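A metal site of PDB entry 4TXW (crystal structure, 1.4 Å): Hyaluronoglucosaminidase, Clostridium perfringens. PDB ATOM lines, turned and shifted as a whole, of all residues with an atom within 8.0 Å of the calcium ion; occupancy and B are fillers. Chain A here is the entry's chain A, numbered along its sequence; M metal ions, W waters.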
ATOM      1  N   ARG A  72      27.665  29.809  16.760  1.00  0.00           N
ATOM      2  CA  ARG A  72      28.082  28.407  16.767  1.00  0.00           C
ATOM      3  C   ARG A  72      27.670  27.653  15.511  1.00  0.00           C
ATOM      4  O   ARG A  72      28.424  26.814  15.015  1.00  0.00           O
ATOM      5  CB  ARG A  72      27.548  27.707  18.010  1.00  0.00           C
ATOM      6  CG  ARG A  72      28.424  27.998  19.230  1.00  0.00           C
ATOM      7  CD  ARG A  72      27.686  27.730  20.505  1.00  0.00           C
ATOM      8  NE  ARG A  72      28.523  27.905  21.677  1.00  0.00           N
ATOM      9  CZ  ARG A  72      28.793  29.072  22.258  1.00  0.00           C
ATOM     10  NH1 ARG A  72      29.548  29.084  23.353  1.00  0.00           N
ATOM     11  NH2 ARG A  72      28.335  30.205  21.756  1.00  0.00           N
ATOM     12  N   ASP A  73      26.496  27.970  14.985  1.00  0.00           N
ATOM     13  CA  ASP A  73      25.978  27.322  13.789  1.00  0.00           C
ATOM     14  C   ASP A  73      25.277  28.348  12.934  1.00  0.00           C
ATOM     15  O   ASP A  73      24.207  28.846  13.278  1.00  0.00           O
ATOM     16  CB  ASP A  73      25.018  26.194  14.144  1.00  0.00           C
ATOM     17  CG  ASP A  73      25.725  24.996  14.753  1.00  0.00           C
ATOM     18  OD1 ASP A  73      26.268  24.192  13.977  1.00  0.00           O
ATOM     19  OD2 ASP A  73      25.773  24.868  15.988  1.00  0.00           O
ATOM     20  N   GLY A  74      25.870  28.689  11.799  1.00  0.00           N
ATOM     21  CA  GLY A  74      25.228  29.649  10.937  1.00  0.00           C
ATOM     22  C   GLY A  74      25.980  29.862   9.657  1.00  0.00           C
ATOM     23  O   GLY A  74      27.064  29.305   9.451  1.00  0.00           O
ATOM     24  N   ILE A  91      29.725  28.416   9.364  1.00  0.00           N
ATOM     25  CA  ILE A  91      30.139  28.260  10.742  1.00  0.00           C
ATOM     26  C   ILE A  91      29.436  27.062  11.341  1.00  0.00           C
ATOM     27  O   ILE A  91      28.196  26.994  11.360  1.00  0.00           O
ATOM     28  CB  ILE A  91      29.782  29.515  11.566  1.00  0.00           C
ATOM     29  CG1 ILE A  91      30.376  30.770  10.926  1.00  0.00           C
ATOM     30  CG2 ILE A  91      30.244  29.352  13.011  1.00  0.00           C
ATOM     31  CD1 ILE A  91      29.955  32.077  11.647  1.00  0.00           C
ATOM     32  N   GLY A  92      30.211  26.112  11.864  1.00  0.00           N
ATOM     33  CA  GLY A  92      29.643  24.938  12.496  1.00  0.00           C
ATOM     34  C   GLY A  92      29.069  23.936  11.507  1.00  0.00           C
ATOM     35  O   GLY A  92      29.343  24.000  10.304  1.00  0.00           O
ATOM     36  N   ASP A  93      28.273  23.021  12.035  1.00  0.00           N
ATOM     37  CA  ASP A  93      27.749  21.906  11.238  1.00  0.00           C
ATOM     38  C   ASP A  93      26.248  21.976  10.993  1.00  0.00           C
ATOM     39  O   ASP A  93      25.675  21.087  10.355  1.00  0.00           O
ATOM     40  CB  ASP A  93      28.117  20.574  11.903  1.00  0.00           C
ATOM     41  CG  ASP A  93      27.494  20.401  13.283  1.00  0.00           C
ATOM     42  OD1 ASP A  93      26.799  21.324  13.768  1.00  0.00           O
ATOM     43  OD2 ASP A  93      27.715  19.347  13.904  1.00  0.00           O
ATOM     44  N   GLY A  94      25.584  23.010  11.514  1.00  0.00           N
ATOM     45  CA  GLY A  94      24.159  23.176  11.325  1.00  0.00           C
ATOM     46  C   GLY A  94      23.306  22.341  12.270  1.00  0.00           C
ATOM     47  O   GLY A  94      22.097  22.243  12.082  1.00  0.00           O
ATOM     48  N   VAL A  95      23.937  21.779  13.287  1.00  0.00           N
ATOM     49  CA  VAL A  95      23.265  20.961  14.285  1.00  0.00           C
ATOM     50  C   VAL A  95      23.459  21.609  15.663  1.00  0.00           C
ATOM     51  O   VAL A  95      24.575  21.982  16.026  1.00  0.00           O
ATOM     52  CB  VAL A  95      23.854  19.527  14.296  1.00  0.00           C
ATOM     53  CG1 VAL A  95      23.102  18.636  15.286  1.00  0.00           C
ATOM     54  CG2 VAL A  95      23.846  18.937  12.890  1.00  0.00           C
ATOM     55  N   GLU A  96      22.377  21.732  16.420  1.00  0.00           N
ATOM     56  CA  GLU A  96      22.400  22.421  17.712  1.00  0.00           C
ATOM     57  C   GLU A  96      23.500  21.886  18.636  1.00  0.00           C
ATOM     58  O   GLU A  96      23.590  20.686  18.866  1.00  0.00           O
ATOM     59  CB  GLU A  96      21.038  22.243  18.373  1.00  0.00           C
ATOM     60  CG  GLU A  96      20.833  23.049  19.627  1.00  0.00           C
ATOM     61  CD  GLU A  96      19.431  22.884  20.193  1.00  0.00           C
ATOM     62  OE1 GLU A  96      18.638  22.100  19.638  1.00  0.00           O
ATOM     63  OE2 GLU A  96      19.131  23.540  21.203  1.00  0.00           O
ATOM     64  N   ASN A  97      24.332  22.795  19.158  1.00  0.00           N
ATOM     65  CA  ASN A  97      25.357  22.421  20.146  1.00  0.00           C
ATOM     66  C   ASN A  97      24.725  22.210  21.517  1.00  0.00           C
ATOM     67  O   ASN A  97      23.632  22.713  21.779  1.00  0.00           O
ATOM     68  CB  ASN A  97      26.436  23.500  20.257  1.00  0.00           C
ATOM     69  CG  ASN A  97      27.389  23.511  19.082  1.00  0.00           C
ATOM     70  OD1 ASN A  97      27.124  22.902  18.042  1.00  0.00           O
ATOM     71  ND2 ASN A  97      28.505  24.214  19.223  1.00  0.00           N
ATOM     72  N   GLY A  98      25.421  21.471  22.374  1.00  0.00           N
ATOM     73  CA  GLY A  98      24.913  21.208  23.708  1.00  0.00           C
ATOM     74  C   GLY A  98      25.244  22.283  24.722  1.00  0.00           C
ATOM     75  O   GLY A  98      26.022  23.213  24.447  1.00  0.00           O
ATOM     76  N   ASP A 101      28.821  23.233  25.674  1.00  0.00           N
ATOM     77  CA  ASP A 101      29.589  24.182  24.865  1.00  0.00           C
ATOM     78  C   ASP A 101      29.400  25.638  25.318  1.00  0.00           C
ATOM     79  O   ASP A 101      29.936  26.564  24.693  1.00  0.00           O
ATOM     80  CB  ASP A 101      29.146  24.048  23.405  1.00  0.00           C
ATOM     81  CG  ASP A 101      30.157  24.612  22.419  1.00  0.00           C
ATOM     82  OD1 ASP A 101      31.349  24.245  22.537  1.00  0.00           O
ATOM     83  OD2 ASP A 101      29.775  25.392  21.520  1.00  0.00           O
ATOM     84  N   ASN A 109      35.153  26.240  18.300  1.00  0.00           N
ATOM     85  CA  ASN A 109      34.171  26.106  17.231  1.00  0.00           C
ATOM     86  C   ASN A 109      34.697  26.522  15.861  1.00  0.00           C
ATOM     87  O   ASN A 109      33.951  26.998  15.003  1.00  0.00           O
ATOM     88  CB  ASN A 109      32.888  26.838  17.606  1.00  0.00           C
ATOM     89  CG  ASN A 109      32.089  26.081  18.612  1.00  0.00           C
ATOM     90  OD1 ASN A 109      31.807  24.899  18.401  1.00  0.00           O
ATOM     91  ND2 ASN A 109      31.748  26.712  19.717  1.00  0.00           N
ATOM     92  N   THR A 145      21.577  28.547  11.560  1.00  0.00           N
ATOM     93  CA  THR A 145      21.139  27.293  10.941  1.00  0.00           C
ATOM     94  C   THR A 145      20.741  26.253  11.974  1.00  0.00           C
ATOM     95  O   THR A 145      20.315  25.143  11.616  1.00  0.00           O
ATOM     96  CB  THR A 145      22.228  26.726  10.049  1.00  0.00           C
ATOM     97  OG1 THR A 145      23.449  26.660  10.800  1.00  0.00           O
ATOM     98  CG2 THR A 145      22.434  27.638   8.820  1.00  0.00           C
ATOM     99  N   ALA A 146      20.872  26.625  13.246  1.00  0.00           N
ATOM    100  CA  ALA A 146      20.411  25.815  14.351  1.00  0.00           C
ATOM    101  C   ALA A 146      20.214  26.764  15.535  1.00  0.00           C
ATOM    102  O   ALA A 146      20.758  27.862  15.529  1.00  0.00           O
ATOM    103  CB  ALA A 146      21.443  24.736  14.679  1.00  0.00           C
ATOM    104  N   PRO A 147      19.436  26.351  16.538  1.00  0.00           N
ATOM    105  CA  PRO A 147      19.331  27.216  17.714  1.00  0.00           C
ATOM    106  C   PRO A 147      20.591  27.099  18.544  1.00  0.00           C
ATOM    107  O   PRO A 147      21.339  26.135  18.385  1.00  0.00           O
ATOM    108  CB  PRO A 147      18.168  26.578  18.503  1.00  0.00           C
ATOM    109  CG  PRO A 147      17.587  25.498  17.618  1.00  0.00           C
ATOM    110  CD  PRO A 147      18.666  25.104  16.678  1.00  0.00           C
ATOM    111  N   TYR A 148      20.827  28.077  19.405  1.00  0.00           N
ATOM    112  CA  TYR A 148      21.679  27.831  20.555  1.00  0.00           C
ATOM    113  C   TYR A 148      21.095  28.614  21.713  1.00  0.00           C
ATOM    114  O   TYR A 148      21.201  29.833  21.768  1.00  0.00           O
ATOM    115  CB  TYR A 148      23.144  28.209  20.308  1.00  0.00           C
ATOM    116  CG  TYR A 148      24.000  27.643  21.419  1.00  0.00           C
ATOM    117  CD1 TYR A 148      24.066  26.273  21.634  1.00  0.00           C
ATOM    118  CD2 TYR A 148      24.691  28.477  22.296  1.00  0.00           C
ATOM    119  CE1 TYR A 148      24.812  25.732  22.669  1.00  0.00           C
ATOM    120  CE2 TYR A 148      25.440  27.944  23.334  1.00  0.00           C
ATOM    121  CZ  TYR A 148      25.486  26.572  23.534  1.00  0.00           C
ATOM    122  OH  TYR A 148      26.230  26.021  24.567  1.00  0.00           O
HETATM  123 CA    CA M   1      26.764  22.600  15.774  1.00  0.00          CA
HETATM  124  O   HOH W   1      29.016  22.830  15.154  1.00  0.00           O
HETATM  125  O   HOH W   2      27.401  20.318  16.513  1.00  0.00           O
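The calcium ion is bound by O of Val 95 (2.3 Å), OD1 of Asn 97 (2.3 Å), water W1 (2.3 Å), OD1 of Asp 93 (2.4 Å), OD1 of Asp 73 (2.5 Å), water W2 (2.5 Å) and OD2 of Asp 73 (2.5 Å). The calcium ion has seven donor atoms within binding distance.
The side-chain amide nitrogen (ND2) of Asn 97 sits at hydrogen-bond distance from the side-chain amide oxygen (OD1) of Asn 109 (3.5 Å). ND2 of Asn 97 is in hydrogen-bond range of OD2 of Asp 101, 2.9 Å away. OD1 of Asp 73 lies close to N of Gly 94, 2.8 Å away. The backbone carbonyl oxygen (O) of Asp 73 sits at hydrogen-bond distance from the backbone NH (N) of Thr 145.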
